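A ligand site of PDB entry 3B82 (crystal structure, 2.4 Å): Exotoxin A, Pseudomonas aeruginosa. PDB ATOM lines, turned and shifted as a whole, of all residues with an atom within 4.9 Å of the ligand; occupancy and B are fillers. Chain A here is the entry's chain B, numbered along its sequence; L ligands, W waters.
The side-chain amide oxygen (OE1) of Gln 62 sits at hydrogen-bond distance from the indole nitrogen (NE1) of Trp 160 (3.2 Å).
N of Gly 70 is in hydrogen-bond range of OE1 of Gln 62 (2.7 Å).
NE of Arg 60 is in hydrogen-bond range of O of Arg 58, at 3.3 Å.
O of Ser 51 is in hydrogen-bond range of N of Gly 56.
A ring nitrogen (ND1) of His 42 lies within hydrogen-bond range of the backbone carbonyl oxygen (O) of Tyr 72 (2.8 Å).
O of Ala 74 sits at hydrogen-bond distance from N of Tyr 41 (2.6 Å).
CB of Ala 48 touches C6 of the ligand, 3.5 Å away.
Ile 52 touches the ligand (CG1 to C7, 3.6 Å).
Val 57 touches the ligand (CA to N4, 3.4 Å).
CE1 of Phe 71 touches C9 of the ligand, 3.8 Å away.
Tyr 72 touches the ligand (CD2 to C14, 3.3 Å).
Ile 73 touches the ligand.
Ala 74 touches the ligand.
CB of Ala 80 touches O14 of the ligand, at 3.6 Å.
Hydrophobic or aromatic side chains that line the ligand: His 42, Ala 48, Ile 52, Val 57, Phe 71, Tyr 72, Ala 80 and Tyr 83.
Within 4 Å of the ligand: His 42, Gly 43, Thr 44, Ala 48, Ser 51, Ile 52, Gly 56, Val 57, Arg 58, Arg 60, Gln 62, Phe 71, Tyr 72, Ile 73, Ala 74, Ala 80, Tyr 83 and Glu 155.
Along chain A the residues within 4 Å of the ligand span positions 42 to 155.
The nearest printed residue that does not touch the ligand is Tyr 41 (4.1 Å).
Water W3 lies within hydrogen-bond range of O5 of the ligand, O of Gly 43 and OG1 of Thr 44.
Water W1 bridges O8 of the ligand (2.6 Å) and N of Tyr 72 (3.0 Å).
Water W4 bridges an oxygen (O12) of the ligand and the side-chain hydroxyl of Tyr 72.
Water W6 lies within hydrogen-bond range of O of Gly 56, O of Ser 51 and N3 of the ligand.
The side-chain hydroxyl (OG1) of Thr 44 is in hydrogen-bond range of an oxygen (O6) of the ligand.
NE2 of Gln 62 lies within hydrogen-bond range of O2 of the ligand (2.8 Å).
The side-chain carboxylate (OE1) of Glu 155 is in hydrogen-bond range of an oxygen (O13) of the ligand, 2.8 Å away.
N of Arg 58 sits at hydrogen-bond distance from N4 of the ligand.
N of Gly 43 sits at hydrogen-bond distance from O14 of the ligand, 2.9 Å away.
N7 of the ligand sits at hydrogen-bond distance from O of Gly 43 (3.2 Å).
N3 of the ligand lies within hydrogen-bond range of O of Gly 56 (3.0 Å).
O6 of the ligand sits at hydrogen-bond distance from NE2 of His 42.
N3 of the ligand is in hydrogen-bond range of OG of Ser 51.
The guanidinium group of Arg 60 sits close to a nitrogen (N5) of the ligand (3.2 Å).
An oxygen (O11) of the ligand lies close to the side-chain hydroxyl of Tyr 83, at 3.4 Å.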
ATOM      1  N   TYR A  41      -9.524  25.714 -36.409  1.00  0.00           N
ATOM      2  CA  TYR A  41     -10.180  24.450 -36.076  1.00  0.00           C
ATOM      3  C   TYR A  41     -10.440  24.311 -34.584  1.00  0.00           C
ATOM      4  O   TYR A  41      -9.700  24.849 -33.755  1.00  0.00           O
ATOM      5  CB  TYR A  41      -9.305  23.283 -36.532  1.00  0.00           C
ATOM      6  CG  TYR A  41      -9.217  23.101 -38.027  1.00  0.00           C
ATOM      7  CD1 TYR A  41     -10.127  22.293 -38.706  1.00  0.00           C
ATOM      8  CD2 TYR A  41      -8.209  23.724 -38.763  1.00  0.00           C
ATOM      9  CE1 TYR A  41     -10.039  22.120 -40.076  1.00  0.00           C
ATOM     10  CE2 TYR A  41      -8.119  23.559 -40.128  1.00  0.00           C
ATOM     11  CZ  TYR A  41      -9.032  22.759 -40.778  1.00  0.00           C
ATOM     12  OH  TYR A  41      -8.953  22.587 -42.145  1.00  0.00           O
ATOM     13  N   HIS A  42     -11.495  23.567 -34.243  1.00  0.00           N
ATOM     14  CA  HIS A  42     -11.775  23.203 -32.869  1.00  0.00           C
ATOM     15  C   HIS A  42     -12.085  21.711 -32.779  1.00  0.00           C
ATOM     16  O   HIS A  42     -13.020  21.230 -33.411  1.00  0.00           O
ATOM     17  CB  HIS A  42     -12.948  24.011 -32.314  1.00  0.00           C
ATOM     18  CG  HIS A  42     -13.353  23.612 -30.920  1.00  0.00           C
ATOM     19  ND1 HIS A  42     -12.807  24.182 -29.792  1.00  0.00           N
ATOM     20  CD2 HIS A  42     -14.256  22.700 -30.493  1.00  0.00           C
ATOM     21  CE1 HIS A  42     -13.361  23.636 -28.723  1.00  0.00           C
ATOM     22  NE2 HIS A  42     -14.237  22.742 -29.116  1.00  0.00           N
ATOM     23  N   GLY A  43     -11.272  20.987 -32.007  1.00  0.00           N
ATOM     24  CA  GLY A  43     -11.486  19.562 -31.816  1.00  0.00           C
ATOM     25  C   GLY A  43     -12.174  19.265 -30.497  1.00  0.00           C
ATOM     26  O   GLY A  43     -11.865  19.887 -29.481  1.00  0.00           O
ATOM     27  N   THR A  44     -13.105  18.319 -30.519  1.00  0.00           N
ATOM     28  CA  THR A  44     -13.870  17.976 -29.326  1.00  0.00           C
ATOM     29  C   THR A  44     -14.613  16.647 -29.501  1.00  0.00           C
ATOM     30  O   THR A  44     -14.505  16.005 -30.541  1.00  0.00           O
ATOM     31  CB  THR A  44     -14.878  19.095 -28.965  1.00  0.00           C
ATOM     32  OG1 THR A  44     -15.402  18.862 -27.652  1.00  0.00           O
ATOM     33  CG2 THR A  44     -16.014  19.131 -29.979  1.00  0.00           C
ATOM     34  N   PHE A  45     -15.373  16.262 -28.479  1.00  0.00           N
ATOM     35  CA  PHE A  45     -16.115  15.010 -28.522  1.00  0.00           C
ATOM     36  C   PHE A  45     -17.468  15.145 -29.238  1.00  0.00           C
ATOM     37  O   PHE A  45     -17.977  16.254 -29.398  1.00  0.00           O
ATOM     38  CB  PHE A  45     -16.296  14.418 -27.116  1.00  0.00           C
ATOM     39  CG  PHE A  45     -16.979  15.351 -26.144  1.00  0.00           C
ATOM     40  CD1 PHE A  45     -16.297  16.414 -25.580  1.00  0.00           C
ATOM     41  CD2 PHE A  45     -18.304  15.140 -25.780  1.00  0.00           C
ATOM     42  CE1 PHE A  45     -16.918  17.251 -24.677  1.00  0.00           C
ATOM     43  CE2 PHE A  45     -18.936  15.984 -24.884  1.00  0.00           C
ATOM     44  CZ  PHE A  45     -18.248  17.043 -24.336  1.00  0.00           C
ATOM     45  N   ALA A  48     -20.387  17.290 -27.934  1.00  0.00           N
ATOM     46  CA  ALA A  48     -20.013  18.690 -27.960  1.00  0.00           C
ATOM     47  C   ALA A  48     -20.102  19.235 -29.381  1.00  0.00           C
ATOM     48  O   ALA A  48     -20.540  20.360 -29.601  1.00  0.00           O
ATOM     49  CB  ALA A  48     -18.610  18.877 -27.404  1.00  0.00           C
ATOM     50  N   SER A  51     -23.674  19.867 -30.181  1.00  0.00           N
ATOM     51  CA  SER A  51     -24.089  21.076 -29.475  1.00  0.00           C
ATOM     52  C   SER A  51     -23.605  22.337 -30.181  1.00  0.00           C
ATOM     53  O   SER A  51     -24.361  23.278 -30.403  1.00  0.00           O
ATOM     54  CB  SER A  51     -23.570  21.050 -28.044  1.00  0.00           C
ATOM     55  OG  SER A  51     -23.686  22.327 -27.433  1.00  0.00           O
ATOM     56  N   ILE A  52     -22.326  22.345 -30.525  1.00  0.00           N
ATOM     57  CA  ILE A  52     -21.678  23.514 -31.097  1.00  0.00           C
ATOM     58  C   ILE A  52     -22.214  23.872 -32.492  1.00  0.00           C
ATOM     59  O   ILE A  52     -22.419  25.034 -32.805  1.00  0.00           O
ATOM     60  CB  ILE A  52     -20.150  23.337 -31.153  1.00  0.00           C
ATOM     61  CG1 ILE A  52     -19.556  23.437 -29.747  1.00  0.00           C
ATOM     62  CG2 ILE A  52     -19.513  24.363 -32.080  1.00  0.00           C
ATOM     63  CD1 ILE A  52     -18.141  22.910 -29.628  1.00  0.00           C
ATOM     64  N   GLY A  56     -24.935  26.232 -31.318  1.00  0.00           N
ATOM     65  CA  GLY A  56     -24.030  27.370 -31.264  1.00  0.00           C
ATOM     66  C   GLY A  56     -23.043  27.307 -30.115  1.00  0.00           C
ATOM     67  O   GLY A  56     -23.294  26.648 -29.102  1.00  0.00           O
ATOM     68  N   VAL A  57     -21.922  27.995 -30.274  1.00  0.00           N
ATOM     69  CA  VAL A  57     -20.922  28.091 -29.216  1.00  0.00           C
ATOM     70  C   VAL A  57     -21.451  28.930 -28.061  1.00  0.00           C
ATOM     71  O   VAL A  57     -21.756  30.107 -28.231  1.00  0.00           O
ATOM     72  CB  VAL A  57     -19.623  28.727 -29.733  1.00  0.00           C
ATOM     73  CG1 VAL A  57     -18.670  29.002 -28.589  1.00  0.00           C
ATOM     74  CG2 VAL A  57     -18.974  27.829 -30.786  1.00  0.00           C
ATOM     75  N   ARG A  58     -21.577  28.307 -26.888  1.00  0.00           N
ATOM     76  CA  ARG A  58     -22.068  29.010 -25.707  1.00  0.00           C
ATOM     77  C   ARG A  58     -21.072  28.986 -24.546  1.00  0.00           C
ATOM     78  O   ARG A  58     -20.397  27.981 -24.318  1.00  0.00           O
ATOM     79  CB  ARG A  58     -23.424  28.457 -25.260  1.00  0.00           C
ATOM     80  CG  ARG A  58     -24.619  29.113 -25.938  1.00  0.00           C
ATOM     81  CD  ARG A  58     -24.732  28.708 -27.405  1.00  0.00           C
ATOM     82  NE  ARG A  58     -25.795  29.444 -28.098  1.00  0.00           N
ATOM     83  CZ  ARG A  58     -25.585  30.450 -28.929  1.00  0.00           C
ATOM     84  NH1 ARG A  58     -26.619  31.063 -29.514  1.00  0.00           N
ATOM     85  NH2 ARG A  58     -24.354  30.860 -29.199  1.00  0.00           N
ATOM     86  N   ARG A  60     -19.202  28.729 -21.024  1.00  0.00           N
ATOM     87  CA  ARG A  60     -19.260  27.689 -20.009  1.00  0.00           C
ATOM     88  C   ARG A  60     -18.051  27.793 -19.083  1.00  0.00           C
ATOM     89  O   ARG A  60     -17.023  28.340 -19.463  1.00  0.00           O
ATOM     90  CB  ARG A  60     -19.282  26.311 -20.665  1.00  0.00           C
ATOM     91  CG  ARG A  60     -18.119  26.066 -21.610  1.00  0.00           C
ATOM     92  CD  ARG A  60     -18.381  24.888 -22.523  1.00  0.00           C
ATOM     93  NE  ARG A  60     -19.689  24.987 -23.161  1.00  0.00           N
ATOM     94  CZ  ARG A  60     -20.735  24.241 -22.822  1.00  0.00           C
ATOM     95  NH1 ARG A  60     -20.629  23.341 -21.859  1.00  0.00           N
ATOM     96  NH2 ARG A  60     -21.900  24.394 -23.457  1.00  0.00           N
ATOM     97  N   GLN A  62     -14.787  26.703 -17.456  1.00  0.00           N
ATOM     98  CA  GLN A  62     -13.683  25.846 -17.877  1.00  0.00           C
ATOM     99  C   GLN A  62     -12.560  25.824 -16.840  1.00  0.00           C
ATOM    100  O   GLN A  62     -12.451  26.738 -16.015  1.00  0.00           O
ATOM    101  CB  GLN A  62     -13.152  26.291 -19.247  1.00  0.00           C
ATOM    102  CG  GLN A  62     -12.897  27.784 -19.351  1.00  0.00           C
ATOM    103  CD  GLN A  62     -12.954  28.280 -20.784  1.00  0.00           C
ATOM    104  OE1 GLN A  62     -13.074  29.481 -21.024  1.00  0.00           O
ATOM    105  NE2 GLN A  62     -12.875  27.363 -21.734  1.00  0.00           N
ATOM    106  N   ASP A  63     -11.735  24.797 -16.887  1.00  0.00           N
ATOM    107  CA  ASP A  63     -10.695  24.595 -15.871  1.00  0.00           C
ATOM    108  C   ASP A  63      -9.418  25.373 -16.174  1.00  0.00           C
ATOM    109  O   ASP A  63      -8.426  24.814 -16.638  1.00  0.00           O
ATOM    110  CB  ASP A  63     -10.388  23.101 -15.715  1.00  0.00           C
ATOM    111  CG  ASP A  63      -9.706  22.793 -14.393  1.00  0.00           C
ATOM    112  OD1 ASP A  63      -8.989  23.668 -13.871  1.00  0.00           O
ATOM    113  OD2 ASP A  63      -9.896  21.663 -13.884  1.00  0.00           O
ATOM    114  N   LEU A  64      -9.456  26.676 -15.905  1.00  0.00           N
ATOM    115  CA  LEU A  64      -8.293  27.541 -16.039  1.00  0.00           C
ATOM    116  C   LEU A  64      -8.502  28.824 -15.255  1.00  0.00           C
ATOM    117  O   LEU A  64      -9.525  28.977 -14.581  1.00  0.00           O
ATOM    118  CB  LEU A  64      -8.004  27.843 -17.515  1.00  0.00           C
ATOM    119  CG  LEU A  64      -9.177  28.108 -18.472  1.00  0.00           C
ATOM    120  CD1 LEU A  64      -9.988  29.316 -18.034  1.00  0.00           C
ATOM    121  CD2 LEU A  64      -8.677  28.280 -19.893  1.00  0.00           C
ATOM    122  N   GLY A  70     -12.304  31.571 -22.483  1.00  0.00           N
ATOM    123  CA  GLY A  70     -12.733  31.832 -23.847  1.00  0.00           C
ATOM    124  C   GLY A  70     -12.836  30.545 -24.637  1.00  0.00           C
ATOM    125  O   GLY A  70     -12.750  29.453 -24.082  1.00  0.00           O
ATOM    126  N   PHE A  71     -13.024  30.672 -25.954  1.00  0.00           N
ATOM    127  CA  PHE A  71     -13.159  29.521 -26.832  1.00  0.00           C
ATOM    128  C   PHE A  71     -11.844  29.257 -27.559  1.00  0.00           C
ATOM    129  O   PHE A  71     -11.341  30.137 -28.261  1.00  0.00           O
ATOM    130  CB  PHE A  71     -14.294  29.751 -27.828  1.00  0.00           C
ATOM    131  CG  PHE A  71     -14.677  28.528 -28.609  1.00  0.00           C
ATOM    132  CD1 PHE A  71     -15.249  27.438 -27.985  1.00  0.00           C
ATOM    133  CD2 PHE A  71     -14.480  28.474 -29.990  1.00  0.00           C
ATOM    134  CE1 PHE A  71     -15.615  26.308 -28.708  1.00  0.00           C
ATOM    135  CE2 PHE A  71     -14.844  27.352 -30.708  1.00  0.00           C
ATOM    136  CZ  PHE A  71     -15.400  26.272 -30.067  1.00  0.00           C
ATOM    137  N   TYR A  72     -11.291  28.067 -27.385  1.00  0.00           N
ATOM    138  CA  TYR A  72      -9.981  27.753 -27.929  1.00  0.00           C
ATOM    139  C   TYR A  72     -10.031  27.034 -29.283  1.00  0.00           C
ATOM    140  O   TYR A  72     -10.733  26.034 -29.445  1.00  0.00           O
ATOM    141  CB  TYR A  72      -9.167  26.934 -26.918  1.00  0.00           C
ATOM    142  CG  TYR A  72      -8.689  27.748 -25.744  1.00  0.00           C
ATOM    143  CD1 TYR A  72      -9.549  28.063 -24.700  1.00  0.00           C
ATOM    144  CD2 TYR A  72      -7.381  28.205 -25.670  1.00  0.00           C
ATOM    145  CE1 TYR A  72      -9.123  28.815 -23.618  1.00  0.00           C
ATOM    146  CE2 TYR A  72      -6.939  28.952 -24.606  1.00  0.00           C
ATOM    147  CZ  TYR A  72      -7.815  29.257 -23.578  1.00  0.00           C
ATOM    148  OH  TYR A  72      -7.381  29.999 -22.503  1.00  0.00           O
ATOM    149  N   ILE A  73      -9.275  27.574 -30.240  1.00  0.00           N
ATOM    150  CA  ILE A  73      -9.184  26.988 -31.565  1.00  0.00           C
ATOM    151  C   ILE A  73      -7.740  27.011 -32.054  1.00  0.00           C
ATOM    152  O   ILE A  73      -6.899  27.701 -31.465  1.00  0.00           O
ATOM    153  CB  ILE A  73     -10.062  27.750 -32.591  1.00  0.00           C
ATOM    154  CG1 ILE A  73      -9.457  29.120 -32.896  1.00  0.00           C
ATOM    155  CG2 ILE A  73     -11.487  27.885 -32.074  1.00  0.00           C
ATOM    156  CD1 ILE A  73     -10.214  29.901 -33.951  1.00  0.00           C
ATOM    157  N   ALA A  74      -7.452  26.263 -33.103  1.00  0.00           N
ATOM    158  CA  ALA A  74      -6.106  26.227 -33.665  1.00  0.00           C
ATOM    159  C   ALA A  74      -6.138  26.393 -35.182  1.00  0.00           C
ATOM    160  O   ALA A  74      -6.999  25.845 -35.856  1.00  0.00           O
ATOM    161  CB  ALA A  74      -5.412  24.917 -33.301  1.00  0.00           C
ATOM    162  N   LEU A  79      -3.121  20.385 -34.256  1.00  0.00           N
ATOM    163  CA  LEU A  79      -3.189  20.784 -32.851  1.00  0.00           C
ATOM    164  C   LEU A  79      -4.587  20.552 -32.299  1.00  0.00           C
ATOM    165  O   LEU A  79      -4.745  19.991 -31.213  1.00  0.00           O
ATOM    166  CB  LEU A  79      -2.784  22.247 -32.697  1.00  0.00           C
ATOM    167  CG  LEU A  79      -2.937  22.831 -31.281  1.00  0.00           C
ATOM    168  CD1 LEU A  79      -2.119  22.034 -30.269  1.00  0.00           C
ATOM    169  CD2 LEU A  79      -2.542  24.292 -31.259  1.00  0.00           C
ATOM    170  N   ALA A  80      -5.595  21.005 -33.027  1.00  0.00           N
ATOM    171  CA  ALA A  80      -6.987  20.833 -32.617  1.00  0.00           C
ATOM    172  C   ALA A  80      -7.383  19.364 -32.645  1.00  0.00           C
ATOM    173  O   ALA A  80      -8.283  18.938 -31.929  1.00  0.00           O
ATOM    174  CB  ALA A  80      -7.901  21.656 -33.527  1.00  0.00           C
ATOM    175  N   TYR A  83      -7.496  17.134 -29.453  1.00  0.00           N
ATOM    176  CA  TYR A  83      -8.572  17.304 -28.484  1.00  0.00           C
ATOM    177  C   TYR A  83      -9.887  16.713 -28.990  1.00  0.00           C
ATOM    178  O   TYR A  83     -10.893  16.705 -28.278  1.00  0.00           O
ATOM    179  CB  TYR A  83      -8.754  18.790 -28.149  1.00  0.00           C
ATOM    180  CG  TYR A  83      -7.494  19.455 -27.659  1.00  0.00           C
ATOM    181  CD1 TYR A  83      -7.070  19.308 -26.341  1.00  0.00           C
ATOM    182  CD2 TYR A  83      -6.718  20.233 -28.502  1.00  0.00           C
ATOM    183  CE1 TYR A  83      -5.919  19.916 -25.884  1.00  0.00           C
ATOM    184  CE2 TYR A  83      -5.568  20.847 -28.054  1.00  0.00           C
ATOM    185  CZ  TYR A  83      -5.159  20.685 -26.743  1.00  0.00           C
ATOM    186  OH  TYR A  83      -4.012  21.290 -26.300  1.00  0.00           O
ATOM    187  N   GLU A 155      -2.184  28.704 -31.008  1.00  0.00           N
ATOM    188  CA  GLU A 155      -3.592  28.547 -30.634  1.00  0.00           C
ATOM    189  C   GLU A 155      -4.264  29.920 -30.637  1.00  0.00           C
ATOM    190  O   GLU A 155      -3.622  30.932 -30.388  1.00  0.00           O
ATOM    191  CB  GLU A 155      -3.726  27.900 -29.259  1.00  0.00           C
ATOM    192  CG  GLU A 155      -3.323  28.796 -28.105  1.00  0.00           C
ATOM    193  CD  GLU A 155      -3.585  28.162 -26.751  1.00  0.00           C
ATOM    194  OE1 GLU A 155      -4.183  27.062 -26.715  1.00  0.00           O
ATOM    195  OE2 GLU A 155      -3.184  28.750 -25.722  1.00  0.00           O
ATOM    196  N   TRP A 160     -15.305  35.039 -25.167  1.00  0.00           N
ATOM    197  CA  TRP A 160     -16.628  34.413 -25.154  1.00  0.00           C
ATOM    198  C   TRP A 160     -17.694  35.188 -25.930  1.00  0.00           C
ATOM    199  O   TRP A 160     -18.467  34.590 -26.684  1.00  0.00           O
ATOM    200  CB  TRP A 160     -17.094  34.108 -23.728  1.00  0.00           C
ATOM    201  CG  TRP A 160     -16.558  32.808 -23.204  1.00  0.00           C
ATOM    202  CD1 TRP A 160     -15.811  32.622 -22.075  1.00  0.00           C
ATOM    203  CD2 TRP A 160     -16.719  31.511 -23.788  1.00  0.00           C
ATOM    204  NE1 TRP A 160     -15.501  31.296 -21.919  1.00  0.00           N
ATOM    205  CE2 TRP A 160     -16.045  30.587 -22.957  1.00  0.00           C
ATOM    206  CE3 TRP A 160     -17.368  31.041 -24.933  1.00  0.00           C
ATOM    207  CZ2 TRP A 160     -15.998  29.229 -23.240  1.00  0.00           C
ATOM    208  CZ3 TRP A 160     -17.321  29.683 -25.216  1.00  0.00           C
ATOM    209  CH2 TRP A 160     -16.647  28.794 -24.362  1.00  0.00           C
HETATM  210  P1  LIG L   1     -12.476  23.757 -22.567  1.00  0.00           P
HETATM  211  O1  LIG L   1     -12.513  23.450 -21.082  1.00  0.00           O
HETATM  212  O2  LIG L   1     -11.905  25.076 -23.032  1.00  0.00           O
HETATM  213  O3  LIG L   1     -13.999  23.640 -23.061  1.00  0.00           O
HETATM  214  C1  LIG L   1     -14.819  22.605 -22.510  1.00  0.00           C
HETATM  215  C2  LIG L   1     -15.543  21.787 -23.580  1.00  0.00           C
HETATM  216  O4  LIG L   1     -16.939  22.079 -23.698  1.00  0.00           O
HETATM  217  C3  LIG L   1     -14.955  21.903 -24.990  1.00  0.00           C
HETATM  218  O5  LIG L   1     -14.321  20.674 -25.369  1.00  0.00           O
HETATM  219  C4  LIG L   1     -16.140  22.157 -25.904  1.00  0.00           C
HETATM  220  O6  LIG L   1     -16.080  21.352 -27.090  1.00  0.00           O
HETATM  221  C5  LIG L   1     -17.323  21.763 -25.045  1.00  0.00           C
HETATM  222  N1  LIG L   1     -18.616  22.352 -25.524  1.00  0.00           N
HETATM  223  C6  LIG L   1     -19.751  21.650 -25.636  1.00  0.00           C
HETATM  224  N2  LIG L   1     -20.726  22.458 -26.091  1.00  0.00           N
HETATM  225  C7  LIG L   1     -20.204  23.685 -26.261  1.00  0.00           C
HETATM  226  C8  LIG L   1     -20.743  24.884 -26.695  1.00  0.00           C
HETATM  227  N3  LIG L   1     -22.053  24.929 -27.043  1.00  0.00           N
HETATM  228  N4  LIG L   1     -19.947  25.967 -26.757  1.00  0.00           N
HETATM  229  C9  LIG L   1     -18.661  25.889 -26.403  1.00  0.00           C
HETATM  230  N5  LIG L   1     -18.105  24.738 -25.976  1.00  0.00           N
HETATM  231  C10 LIG L   1     -18.858  23.623 -25.882  1.00  0.00           C
HETATM  232  O7  LIG L   1     -11.683  22.595 -23.331  1.00  0.00           O
HETATM  233  P2  LIG L   1     -10.992  22.887 -24.762  1.00  0.00           P
HETATM  234  O8  LIG L   1     -11.820  23.902 -25.513  1.00  0.00           O
HETATM  235  O9  LIG L   1     -10.666  21.571 -25.428  1.00  0.00           O
HETATM  236  O10 LIG L   1      -9.621  23.550 -24.242  1.00  0.00           O
HETATM  237  C11 LIG L   1      -8.654  22.704 -23.619  1.00  0.00           C
HETATM  238  C12 LIG L   1      -7.250  23.262 -23.818  1.00  0.00           C
HETATM  239  O11 LIG L   1      -6.780  22.851 -25.095  1.00  0.00           O
HETATM  240  C13 LIG L   1      -7.189  24.778 -23.748  1.00  0.00           C
HETATM  241  O12 LIG L   1      -6.585  25.162 -22.520  1.00  0.00           O
HETATM  242  C14 LIG L   1      -6.292  25.130 -24.918  1.00  0.00           C
HETATM  243  O13 LIG L   1      -5.051  25.647 -24.414  1.00  0.00           O
HETATM  244  C15 LIG L   1      -6.009  23.867 -25.711  1.00  0.00           C
HETATM  245  N6  LIG L   1      -6.479  24.018 -27.093  1.00  0.00           N
HETATM  246  C16 LIG L   1      -7.581  23.360 -27.492  1.00  0.00           C
HETATM  247  C17 LIG L   1      -8.058  23.479 -28.797  1.00  0.00           C
HETATM  248  C18 LIG L   1      -9.287  22.741 -29.242  1.00  0.00           C
HETATM  249  O14 LIG L   1      -9.445  22.522 -30.439  1.00  0.00           O
HETATM  250  N7  LIG L   1     -10.172  22.331 -28.339  1.00  0.00           N
HETATM  251  C19 LIG L   1      -7.375  24.286 -29.704  1.00  0.00           C
HETATM  252  C20 LIG L   1      -6.233  24.948 -29.272  1.00  0.00           C
HETATM  253  C21 LIG L   1      -5.802  24.791 -27.960  1.00  0.00           C
HETATM  254  O   HOH W   1     -12.965  26.282 -25.722  1.00  0.00           O
HETATM  255  O   HOH W   2     -10.272  19.433 -23.447  1.00  0.00           O
HETATM  256  O   HOH W   3     -12.315  19.956 -26.809  1.00  0.00           O
HETATM  257  O   HOH W   4      -5.212  27.697 -21.873  1.00  0.00           O
HETATM  258  O   HOH W   5      -2.182  24.409 -24.287  1.00  0.00           O
HETATM  259  O   HOH W   6     -25.378  24.981 -27.976  1.00  0.00           O
